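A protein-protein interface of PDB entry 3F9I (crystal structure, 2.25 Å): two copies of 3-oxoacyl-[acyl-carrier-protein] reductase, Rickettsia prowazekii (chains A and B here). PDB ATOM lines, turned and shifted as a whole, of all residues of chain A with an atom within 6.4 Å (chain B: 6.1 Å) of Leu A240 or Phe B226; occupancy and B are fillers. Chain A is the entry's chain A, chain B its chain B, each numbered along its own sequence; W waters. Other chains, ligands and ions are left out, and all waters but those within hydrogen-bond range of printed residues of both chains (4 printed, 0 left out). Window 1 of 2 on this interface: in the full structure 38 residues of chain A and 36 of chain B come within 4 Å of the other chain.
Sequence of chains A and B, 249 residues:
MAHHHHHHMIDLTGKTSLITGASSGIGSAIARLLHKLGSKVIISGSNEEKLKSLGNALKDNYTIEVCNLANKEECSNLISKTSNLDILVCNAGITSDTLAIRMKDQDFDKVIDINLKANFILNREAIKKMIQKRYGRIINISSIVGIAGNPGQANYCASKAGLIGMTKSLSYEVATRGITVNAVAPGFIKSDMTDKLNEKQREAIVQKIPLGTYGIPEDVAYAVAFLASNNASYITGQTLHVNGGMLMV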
ATOM      1  N   MET A   9      20.413   8.245   7.257  1.00  0.00           N
ATOM      2  CA  MET A   9      20.726   6.799   7.106  1.00  0.00           C
ATOM      3  C   MET A   9      22.151   6.508   7.536  1.00  0.00           C
ATOM      4  O   MET A   9      22.351   5.741   8.474  1.00  0.00           O
ATOM      5  CB  MET A   9      20.485   6.325   5.658  1.00  0.00           C
ATOM      6  CG  MET A   9      20.372   4.798   5.557  1.00  0.00           C
ATOM      7  SD  MET A   9      20.090   4.110   3.914  1.00  0.00           S
ATOM      8  CE  MET A   9      21.760   3.727   3.351  1.00  0.00           C
ATOM      9  N   ILE A  10      23.143   7.129   6.895  1.00  0.00           N
ATOM     10  CA  ILE A  10      24.543   6.789   7.181  1.00  0.00           C
ATOM     11  C   ILE A  10      25.142   7.653   8.291  1.00  0.00           C
ATOM     12  O   ILE A  10      25.413   8.825   8.094  1.00  0.00           O
ATOM     13  CB  ILE A  10      25.454   6.996   5.991  1.00  0.00           C
ATOM     14  CG1 ILE A  10      25.059   6.100   4.821  1.00  0.00           C
ATOM     15  CG2 ILE A  10      26.872   6.733   6.445  1.00  0.00           C
ATOM     16  CD1 ILE A  10      25.607   6.602   3.452  1.00  0.00           C
ATOM     17  N   ASN A 182      35.747  -4.718   1.413  1.00  0.00           N
ATOM     18  CA  ASN A 182      35.161  -4.440   0.118  1.00  0.00           C
ATOM     19  C   ASN A 182      36.037  -3.513  -0.713  1.00  0.00           C
ATOM     20  O   ASN A 182      36.926  -2.883  -0.199  1.00  0.00           O
ATOM     21  CB  ASN A 182      33.808  -3.762   0.236  1.00  0.00           C
ATOM     22  CG  ASN A 182      32.777  -4.594   0.952  1.00  0.00           C
ATOM     23  OD1 ASN A 182      32.252  -5.543   0.380  1.00  0.00           O
ATOM     24  ND2 ASN A 182      32.391  -4.163   2.183  1.00  0.00           N
ATOM     25  N   ALA A 183      35.756  -3.427  -2.008  1.00  0.00           N
ATOM     26  CA  ALA A 183      36.583  -2.653  -2.954  1.00  0.00           C
ATOM     27  C   ALA A 183      35.695  -1.625  -3.633  1.00  0.00           C
ATOM     28  O   ALA A 183      34.555  -1.901  -3.859  1.00  0.00           O
ATOM     29  CB  ALA A 183      37.220  -3.572  -3.993  1.00  0.00           C
ATOM     30  N   VAL A 184      36.185  -0.417  -3.859  1.00  0.00           N
ATOM     31  CA  VAL A 184      35.494   0.507  -4.769  1.00  0.00           C
ATOM     32  C   VAL A 184      36.376   0.638  -5.992  1.00  0.00           C
ATOM     33  O   VAL A 184      37.581   0.828  -5.883  1.00  0.00           O
ATOM     34  CB  VAL A 184      35.199   1.883  -4.158  1.00  0.00           C
ATOM     35  CG1 VAL A 184      34.623   2.783  -5.175  1.00  0.00           C
ATOM     36  CG2 VAL A 184      34.172   1.793  -2.919  1.00  0.00           C
ATOM     37  N   ALA A 185      35.759   0.495  -7.159  1.00  0.00           N
ATOM     38  CA  ALA A 185      36.449   0.618  -8.440  1.00  0.00           C
ATOM     39  C   ALA A 185      35.941   1.811  -9.150  1.00  0.00           C
ATOM     40  O   ALA A 185      34.952   1.726  -9.830  1.00  0.00           O
ATOM     41  CB  ALA A 185      36.152  -0.569  -9.277  1.00  0.00           C
ATOM     42  N   PRO A 186      36.615   2.945  -9.021  1.00  0.00           N
ATOM     43  CA  PRO A 186      36.179   4.054  -9.805  1.00  0.00           C
ATOM     44  C   PRO A 186      36.509   3.853 -11.290  1.00  0.00           C
ATOM     45  O   PRO A 186      37.544   3.247 -11.661  1.00  0.00           O
ATOM     46  CB  PRO A 186      36.997   5.212  -9.258  1.00  0.00           C
ATOM     47  CG  PRO A 186      37.761   4.738  -8.196  1.00  0.00           C
ATOM     48  CD  PRO A 186      37.818   3.253  -8.269  1.00  0.00           C
ATOM     49  N   TYR A 222      30.984   8.805  -1.863  1.00  0.00           N
ATOM     50  CA  TYR A 222      29.659   8.358  -1.516  1.00  0.00           C
ATOM     51  C   TYR A 222      29.562   6.820  -1.338  1.00  0.00           C
ATOM     52  O   TYR A 222      28.929   6.321  -0.396  1.00  0.00           O
ATOM     53  CB  TYR A 222      28.680   8.796  -2.603  1.00  0.00           C
ATOM     54  CG  TYR A 222      27.306   8.286  -2.374  1.00  0.00           C
ATOM     55  CD1 TYR A 222      26.620   8.610  -1.218  1.00  0.00           C
ATOM     56  CD2 TYR A 222      26.685   7.481  -3.284  1.00  0.00           C
ATOM     57  CE1 TYR A 222      25.324   8.151  -0.989  1.00  0.00           C
ATOM     58  CE2 TYR A 222      25.391   7.012  -3.067  1.00  0.00           C
ATOM     59  CZ  TYR A 222      24.730   7.347  -1.915  1.00  0.00           C
ATOM     60  OH  TYR A 222      23.471   6.858  -1.688  1.00  0.00           O
ATOM     61  N   ALA A 223      30.127   6.091  -2.293  1.00  0.00           N
ATOM     62  CA  ALA A 223      30.159   4.637  -2.255  1.00  0.00           C
ATOM     63  C   ALA A 223      30.922   4.187  -1.015  1.00  0.00           C
ATOM     64  O   ALA A 223      30.496   3.262  -0.349  1.00  0.00           O
ATOM     65  CB  ALA A 223      30.856   4.082  -3.505  1.00  0.00           C
ATOM     66  N   VAL A 224      32.048   4.851  -0.741  1.00  0.00           N
ATOM     67  CA  VAL A 224      32.922   4.489   0.365  1.00  0.00           C
ATOM     68  C   VAL A 224      32.171   4.664   1.699  1.00  0.00           C
ATOM     69  O   VAL A 224      32.052   3.705   2.470  1.00  0.00           O
ATOM     70  CB  VAL A 224      34.279   5.257   0.342  1.00  0.00           C
ATOM     71  CG1 VAL A 224      35.114   4.899   1.588  1.00  0.00           C
ATOM     72  CG2 VAL A 224      35.095   4.933  -0.965  1.00  0.00           C
ATOM     73  N   PHE A 226      29.003   4.639   2.273  1.00  0.00           N
ATOM     74  CA  PHE A 226      28.031   3.577   2.410  1.00  0.00           C
ATOM     75  C   PHE A 226      28.703   2.274   2.896  1.00  0.00           C
ATOM     76  O   PHE A 226      28.292   1.667   3.895  1.00  0.00           O
ATOM     77  CB  PHE A 226      27.325   3.335   1.099  1.00  0.00           C
ATOM     78  CG  PHE A 226      26.397   2.196   1.151  1.00  0.00           C
ATOM     79  CD1 PHE A 226      25.302   2.234   2.016  1.00  0.00           C
ATOM     80  CD2 PHE A 226      26.621   1.064   0.398  1.00  0.00           C
ATOM     81  CE1 PHE A 226      24.449   1.145   2.102  1.00  0.00           C
ATOM     82  CE2 PHE A 226      25.784   0.001   0.474  1.00  0.00           C
ATOM     83  CZ  PHE A 226      24.688   0.038   1.332  1.00  0.00           C
ATOM     84  N   LEU A 227      29.767   1.842   2.219  1.00  0.00           N
ATOM     85  CA  LEU A 227      30.386   0.584   2.606  1.00  0.00           C
ATOM     86  C   LEU A 227      31.010   0.671   3.994  1.00  0.00           C
ATOM     87  O   LEU A 227      31.070  -0.321   4.695  1.00  0.00           O
ATOM     88  CB  LEU A 227      31.448   0.201   1.602  1.00  0.00           C
ATOM     89  CG  LEU A 227      30.897  -0.184   0.222  1.00  0.00           C
ATOM     90  CD1 LEU A 227      32.122  -0.296  -0.712  1.00  0.00           C
ATOM     91  CD2 LEU A 227      30.088  -1.456   0.294  1.00  0.00           C
ATOM     92  N   GLN A 238      32.770  -7.535  -1.926  1.00  0.00           N
ATOM     93  CA  GLN A 238      32.208  -7.009  -3.138  1.00  0.00           C
ATOM     94  C   GLN A 238      33.092  -5.913  -3.648  1.00  0.00           C
ATOM     95  O   GLN A 238      33.848  -5.300  -2.892  1.00  0.00           O
ATOM     96  CB  GLN A 238      30.793  -6.504  -2.898  1.00  0.00           C
ATOM     97  CG  GLN A 238      29.922  -7.512  -2.168  1.00  0.00           C
ATOM     98  CD  GLN A 238      29.827  -8.896  -2.838  1.00  0.00           C
ATOM     99  OE1 GLN A 238      29.703  -8.997  -4.049  1.00  0.00           O
ATOM    100  NE2 GLN A 238      29.829  -9.962  -2.023  1.00  0.00           N
ATOM    101  N   THR A 239      33.026  -5.713  -4.958  1.00  0.00           N
ATOM    102  CA  THR A 239      33.651  -4.606  -5.574  1.00  0.00           C
ATOM    103  C   THR A 239      32.496  -3.760  -6.049  1.00  0.00           C
ATOM    104  O   THR A 239      31.580  -4.261  -6.597  1.00  0.00           O
ATOM    105  CB  THR A 239      34.503  -5.024  -6.774  1.00  0.00           C
ATOM    106  OG1 THR A 239      35.498  -5.975  -6.360  1.00  0.00           O
ATOM    107  CG2 THR A 239      35.195  -3.856  -7.310  1.00  0.00           C
ATOM    108  N   LEU A 240      32.548  -2.462  -5.833  1.00  0.00           N
ATOM    109  CA  LEU A 240      31.473  -1.625  -6.289  1.00  0.00           C
ATOM    110  C   LEU A 240      32.068  -0.642  -7.264  1.00  0.00           C
ATOM    111  O   LEU A 240      32.994   0.072  -6.955  1.00  0.00           O
ATOM    112  CB  LEU A 240      30.829  -0.966  -5.091  1.00  0.00           C
ATOM    113  CG  LEU A 240      29.714   0.045  -5.195  1.00  0.00           C
ATOM    114  CD1 LEU A 240      28.686  -0.355  -6.226  1.00  0.00           C
ATOM    115  CD2 LEU A 240      29.114   0.183  -3.770  1.00  0.00           C
ATOM    116  N   HIS A 241      31.533  -0.666  -8.478  1.00  0.00           N
ATOM    117  CA  HIS A 241      32.129   0.043  -9.577  1.00  0.00           C
ATOM    118  C   HIS A 241      31.412   1.328  -9.651  1.00  0.00           C
ATOM    119  O   HIS A 241      30.197   1.333  -9.687  1.00  0.00           O
ATOM    120  CB  HIS A 241      31.947  -0.744 -10.878  1.00  0.00           C
ATOM    121  CG  HIS A 241      32.737  -2.000 -10.918  1.00  0.00           C
ATOM    122  ND1 HIS A 241      34.052  -2.037 -11.345  1.00  0.00           N
ATOM    123  CD2 HIS A 241      32.415  -3.261 -10.549  1.00  0.00           C
ATOM    124  CE1 HIS A 241      34.507  -3.270 -11.235  1.00  0.00           C
ATOM    125  NE2 HIS A 241      33.527  -4.034 -10.771  1.00  0.00           N
ATOM    126  N   VAL A 242      32.153   2.425  -9.682  1.00  0.00           N
ATOM    127  CA  VAL A 242      31.532   3.722  -9.763  1.00  0.00           C
ATOM    128  C   VAL A 242      32.049   4.356 -11.042  1.00  0.00           C
ATOM    129  O   VAL A 242      33.031   5.092 -11.034  1.00  0.00           O
ATOM    130  CB  VAL A 242      31.824   4.599  -8.483  1.00  0.00           C
ATOM    131  CG1 VAL A 242      31.103   5.947  -8.596  1.00  0.00           C
ATOM    132  CG2 VAL A 242      31.415   3.835  -7.200  1.00  0.00           C
ATOM    133  N   ILE B  10      21.025  10.692   1.549  1.00  0.00           N
ATOM    134  CA  ILE B  10      19.957   9.957   0.860  1.00  0.00           C
ATOM    135  C   ILE B  10      18.595  10.583   1.172  1.00  0.00           C
ATOM    136  O   ILE B  10      17.730   9.976   1.796  1.00  0.00           O
ATOM    137  CB  ILE B  10      19.889   8.449   1.240  1.00  0.00           C
ATOM    138  CG1 ILE B  10      21.267   7.756   1.130  1.00  0.00           C
ATOM    139  CG2 ILE B  10      18.894   7.742   0.329  1.00  0.00           C
ATOM    140  CD1 ILE B  10      21.226   6.246   1.453  1.00  0.00           C
ATOM    141  N   ALA B 221      16.999  -3.268   1.886  1.00  0.00           N
ATOM    142  CA  ALA B 221      16.492  -1.912   1.965  1.00  0.00           C
ATOM    143  C   ALA B 221      17.584  -0.847   2.034  1.00  0.00           C
ATOM    144  O   ALA B 221      17.511   0.169   1.358  1.00  0.00           O
ATOM    145  CB  ALA B 221      15.537  -1.794   3.199  1.00  0.00           C
ATOM    146  N   TYR B 222      18.616  -1.070   2.829  1.00  0.00           N
ATOM    147  CA  TYR B 222      19.694  -0.095   2.898  1.00  0.00           C
ATOM    148  C   TYR B 222      20.391   0.010   1.553  1.00  0.00           C
ATOM    149  O   TYR B 222      20.709   1.127   1.080  1.00  0.00           O
ATOM    150  CB  TYR B 222      20.755  -0.491   3.927  1.00  0.00           C
ATOM    151  CG  TYR B 222      20.345  -0.469   5.365  1.00  0.00           C
ATOM    152  CD1 TYR B 222      19.426   0.435   5.843  1.00  0.00           C
ATOM    153  CD2 TYR B 222      20.941  -1.330   6.262  1.00  0.00           C
ATOM    154  CE1 TYR B 222      19.082   0.471   7.181  1.00  0.00           C
ATOM    155  CE2 TYR B 222      20.612  -1.321   7.591  1.00  0.00           C
ATOM    156  CZ  TYR B 222      19.669  -0.425   8.058  1.00  0.00           C
ATOM    157  OH  TYR B 222      19.326  -0.432   9.404  1.00  0.00           O
ATOM    158  N   ALA B 223      20.628  -1.142   0.930  1.00  0.00           N
ATOM    159  CA  ALA B 223      21.281  -1.169  -0.374  1.00  0.00           C
ATOM    160  C   ALA B 223      20.439  -0.444  -1.401  1.00  0.00           C
ATOM    161  O   ALA B 223      20.986   0.305  -2.212  1.00  0.00           O
ATOM    162  CB  ALA B 223      21.545  -2.588  -0.822  1.00  0.00           C
ATOM    163  N   VAL B 224      19.117  -0.647  -1.356  1.00  0.00           N
ATOM    164  CA  VAL B 224      18.178  -0.019  -2.327  1.00  0.00           C
ATOM    165  C   VAL B 224      18.189   1.497  -2.194  1.00  0.00           C
ATOM    166  O   VAL B 224      18.345   2.206  -3.166  1.00  0.00           O
ATOM    167  CB  VAL B 224      16.737  -0.550  -2.127  1.00  0.00           C
ATOM    168  CG1 VAL B 224      15.750   0.179  -3.017  1.00  0.00           C
ATOM    169  CG2 VAL B 224      16.683  -2.053  -2.355  1.00  0.00           C
ATOM    170  N   ALA B 225      18.074   1.973  -0.962  1.00  0.00           N
ATOM    171  CA  ALA B 225      18.192   3.400  -0.596  1.00  0.00           C
ATOM    172  C   ALA B 225      19.489   4.046  -1.083  1.00  0.00           C
ATOM    173  O   ALA B 225      19.530   5.195  -1.519  1.00  0.00           O
ATOM    174  CB  ALA B 225      18.074   3.521   0.960  1.00  0.00           C
ATOM    175  N   PHE B 226      20.583   3.318  -0.947  1.00  0.00           N
ATOM    176  CA  PHE B 226      21.865   3.801  -1.427  1.00  0.00           C
ATOM    177  C   PHE B 226      21.810   4.067  -2.918  1.00  0.00           C
ATOM    178  O   PHE B 226      22.300   5.087  -3.399  1.00  0.00           O
ATOM    179  CB  PHE B 226      22.958   2.777  -1.097  1.00  0.00           C
ATOM    180  CG  PHE B 226      24.269   2.975  -1.843  1.00  0.00           C
ATOM    181  CD1 PHE B 226      25.125   3.982  -1.497  1.00  0.00           C
ATOM    182  CD2 PHE B 226      24.662   2.086  -2.830  1.00  0.00           C
ATOM    183  CE1 PHE B 226      26.300   4.146  -2.140  1.00  0.00           C
ATOM    184  CE2 PHE B 226      25.841   2.228  -3.461  1.00  0.00           C
ATOM    185  CZ  PHE B 226      26.675   3.258  -3.116  1.00  0.00           C
ATOM    186  N   LEU B 227      21.226   3.130  -3.653  1.00  0.00           N
ATOM    187  CA  LEU B 227      21.187   3.245  -5.109  1.00  0.00           C
ATOM    188  C   LEU B 227      20.170   4.314  -5.531  1.00  0.00           C
ATOM    189  O   LEU B 227      20.386   5.046  -6.507  1.00  0.00           O
ATOM    190  CB  LEU B 227      20.823   1.904  -5.730  1.00  0.00           C
ATOM    191  CG  LEU B 227      21.903   0.843  -5.518  1.00  0.00           C
ATOM    192  CD1 LEU B 227      21.407  -0.536  -5.929  1.00  0.00           C
ATOM    193  CD2 LEU B 227      23.133   1.298  -6.250  1.00  0.00           C
ATOM    194  N   ALA B 228      19.070   4.389  -4.765  1.00  0.00           N
ATOM    195  CA  ALA B 228      17.999   5.310  -5.083  1.00  0.00           C
ATOM    196  C   ALA B 228      18.401   6.763  -4.876  1.00  0.00           C
ATOM    197  O   ALA B 228      17.750   7.656  -5.380  1.00  0.00           O
ATOM    198  CB  ALA B 228      16.729   4.968  -4.276  1.00  0.00           C
ATOM    199  N   SER B 229      19.482   7.026  -4.155  1.00  0.00           N
ATOM    200  CA  SER B 229      19.846   8.412  -3.829  1.00  0.00           C
ATOM    201  C   SER B 229      20.261   9.274  -5.015  1.00  0.00           C
ATOM    202  O   SER B 229      20.828   8.785  -6.007  1.00  0.00           O
ATOM    203  CB  SER B 229      20.997   8.415  -2.834  1.00  0.00           C
ATOM    204  OG  SER B 229      21.510   9.715  -2.710  1.00  0.00           O
ATOM    205  N   ASN B 231      22.829  10.935  -4.962  1.00  0.00           N
ATOM    206  CA  ASN B 231      24.277  10.822  -5.041  1.00  0.00           C
ATOM    207  C   ASN B 231      24.769   9.499  -5.684  1.00  0.00           C
ATOM    208  O   ASN B 231      25.970   9.306  -5.860  1.00  0.00           O
ATOM    209  CB  ASN B 231      24.867  11.039  -3.653  1.00  0.00           C
ATOM    210  CG  ASN B 231      24.531  12.403  -3.090  1.00  0.00           C
ATOM    211  OD1 ASN B 231      23.859  12.500  -2.078  1.00  0.00           O
ATOM    212  ND2 ASN B 231      25.021  13.454  -3.724  1.00  0.00           N
ATOM    213  N   ALA B 232      23.851   8.604  -6.035  1.00  0.00           N
ATOM    214  CA  ALA B 232      24.171   7.329  -6.708  1.00  0.00           C
ATOM    215  C   ALA B 232      24.106   7.503  -8.215  1.00  0.00           C
ATOM    216  O   ALA B 232      23.892   6.575  -8.958  1.00  0.00           O
ATOM    217  CB  ALA B 232      23.209   6.289  -6.283  1.00  0.00           C
ATOM    218  N   ILE B 235      26.428   5.653 -10.754  1.00  0.00           N
ATOM    219  CA  ILE B 235      26.438   4.242 -10.528  1.00  0.00           C
ATOM    220  C   ILE B 235      25.304   3.693 -11.295  1.00  0.00           C
ATOM    221  O   ILE B 235      24.157   3.893 -10.916  1.00  0.00           O
ATOM    222  CB  ILE B 235      26.232   3.878  -9.046  1.00  0.00           C
ATOM    223  CG1 ILE B 235      27.441   4.332  -8.227  1.00  0.00           C
ATOM    224  CG2 ILE B 235      25.949   2.340  -8.885  1.00  0.00           C
ATOM    225  CD1 ILE B 235      27.226   4.254  -6.774  1.00  0.00           C
ATOM    226  N   GLN B 238      24.890  -1.906 -12.238  1.00  0.00           N
ATOM    227  CA  GLN B 238      25.668  -2.702 -11.283  1.00  0.00           C
ATOM    228  C   GLN B 238      24.720  -3.580 -10.539  1.00  0.00           C
ATOM    229  O   GLN B 238      23.525  -3.318 -10.484  1.00  0.00           O
ATOM    230  CB  GLN B 238      26.388  -1.800 -10.291  1.00  0.00           C
ATOM    231  CG  GLN B 238      27.256  -0.728 -10.954  1.00  0.00           C
ATOM    232  CD  GLN B 238      28.298  -1.352 -11.837  1.00  0.00           C
ATOM    233  OE1 GLN B 238      28.991  -2.270 -11.411  1.00  0.00           O
ATOM    234  NE2 GLN B 238      28.396  -0.898 -13.070  1.00  0.00           N
ATOM    235  N   THR B 239      25.265  -4.667 -10.010  1.00  0.00           N
ATOM    236  CA  THR B 239      24.546  -5.547  -9.154  1.00  0.00           C
ATOM    237  C   THR B 239      25.202  -5.414  -7.800  1.00  0.00           C
ATOM    238  O   THR B 239      26.366  -5.679  -7.650  1.00  0.00           O
ATOM    239  CB  THR B 239      24.622  -7.000  -9.635  1.00  0.00           C
ATOM    240  OG1 THR B 239      24.281  -7.039 -11.014  1.00  0.00           O
ATOM    241  CG2 THR B 239      23.630  -7.863  -8.874  1.00  0.00           C
ATOM    242  N   LEU B 240      24.434  -5.018  -6.799  1.00  0.00           N
ATOM    243  CA  LEU B 240      24.973  -4.864  -5.453  1.00  0.00           C
ATOM    244  C   LEU B 240      24.575  -6.142  -4.720  1.00  0.00           C
ATOM    245  O   LEU B 240      23.409  -6.393  -4.513  1.00  0.00           O
ATOM    246  CB  LEU B 240      24.421  -3.573  -4.852  1.00  0.00           C
ATOM    247  CG  LEU B 240      24.924  -3.096  -3.482  1.00  0.00           C
ATOM    248  CD1 LEU B 240      26.407  -3.277  -3.314  1.00  0.00           C
ATOM    249  CD2 LEU B 240      24.545  -1.645  -3.221  1.00  0.00           C
ATOM    250  N   VAL B 249      31.167 -10.710  -6.218  1.00  0.00           N
ATOM    251  CA  VAL B 249      31.273 -10.167  -7.589  1.00  0.00           C
ATOM    252  C   VAL B 249      31.747  -8.689  -7.621  1.00  0.00           C
ATOM    253  O   VAL B 249      31.693  -7.948  -6.620  1.00  0.00           O
ATOM    254  CB  VAL B 249      29.908 -10.318  -8.348  1.00  0.00           C
ATOM    255  CG1 VAL B 249      29.897  -9.551  -9.685  1.00  0.00           C
ATOM    256  CG2 VAL B 249      29.576 -11.810  -8.555  1.00  0.00           C
HETATM  257  O   HOH W   1      28.845   2.338 -11.931  1.00  0.00           O
HETATM  258  O   HOH W   2      34.865  -8.221  -5.354  1.00  0.00           O
HETATM  259  O   HOH W   3      29.594  -2.555  -8.975  1.00  0.00           O
HETATM  260  O   HOH W   4      28.480  -6.748  -5.159  1.00  0.00           O
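The backbone carbonyl oxygen of Val B249 is in hydrogen-bond range of the backbone NH of Thr A239 (3.1 Å). The backbone NH (N) of Val B249 lies within hydrogen-bond range of the side-chain amide oxygen (OE1) of Gln A238. The side-chain hydroxyl of Tyr A222 sits at hydrogen-bond distance from the backbone carbonyl oxygen of Phe B226, at 2.7 Å.
O of Ala A183 sits at hydrogen-bond distance from N of Leu A240 (2.9 Å). N of Ala A183 sits at hydrogen-bond distance from O of Gln A238, at 2.8 Å. The backbone NH (N) of Gln A238 lies within hydrogen-bond range of the side-chain amide oxygen (OD1) of Asn A182 (3.1 Å). The backbone NH of Asn B231 lies within hydrogen-bond range of the side-chain hydroxyl of Ser B229, at 2.9 Å. The backbone NH (N) of Ala A185 is in hydrogen-bond range of the backbone carbonyl oxygen (O) of Leu A240 (2.8 Å).
Met A9 touches Ile B10. CE of Met A9 touches O of Tyr B222, at 3.6 Å. Met A9 touches Ala B225 (SD to CB, 3.6 Å). Tyr A222 touches Ile B10. Tyr A222 touches Ala B232 (CE2 to N, 3.7 Å). CZ of Phe B226 touches CA of Ala A223, at 3.8 Å. CE1 of Phe A226 touches O of Tyr B222 (3.9 Å). CG of Phe A226 touches CD1 of Phe B226, 3.4 Å away. Leu A240 touches Phe B226 (CD2 to CE2, 3.9 Å). His A241 touches Gln B238 (CB to OE1, 3.4 Å).
Leu A240 touches just one residue of chain B: Phe B226 (3.9 Å). Of chain A, only Tyr A222 (2.7 Å), Ala A223 (3.8 Å), Phe A226 (3.4 Å) and Leu A240 (3.9 Å) come within 4 Å of Phe B226. Printed residues of chain B within 4 Å of His A241: Gln B238. Printed residues of chain A within 4 Å of Val B249: Gln A238 and Thr A239. Printed residues of chain B within 4 Å of Phe A226: Tyr B222 (3.9 Å), Ala B223 (3.997 Å) and Phe B226 (3.4 Å). Printed residues of chain A within 4 Å of Asn B231: Tyr A222. The nearest residue of chain B that does not touch Leu A240 is Leu B240 (4.4 Å).
Hydrophobic or aromatic side chains of chain A within 4 Å of the printed part of chain B: Met A9, Tyr A222, Phe A226, Leu A240 and His A241. Hydrophobic or aromatic side chains of chain B that line the printed part of chain A: Ile B10, Ala B225, Phe B226 and Ala B232. Among the printed residues, 16 pairs touch across the chains. Among the printed residues, no Asp or Glu carboxylate lies within 4 Å of a Lys or Arg side-chain nitrogen of the other chain.
Tyr A222 touches Ile B10, but with the chains exchanged Ile A10 does not touch Tyr B222 (7.6 Å). Ala A223 touches Phe B226, and with the chains exchanged Phe A226 touches Ala B223. Phe A226 touches its own counterpart, Phe B226. Leu A240 touches Phe B226, but with the chains exchanged Phe A226 does not touch Leu B240 (4.2 Å). 9 positions are printed for both chains.
Water W3 lies within hydrogen-bond range of the side-chain amide oxygen (OE1) of Gln B238 (2.5 Å) and the backbone NH (N) of His A241 (2.8 Å). Water W2 bridges OG1 of Thr A239 (2.5 Å) and O of Val B249 (3.4 Å). Water W4 bridges the side-chain amide oxygen (OE1) of Gln A238 (2.8 Å) and the backbone carbonyl oxygen (O) of Thr B239 (3.4 Å). Water W1 bridges O of His A241 (2.8 Å) and NE2 of Gln B238 (3.5 Å).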
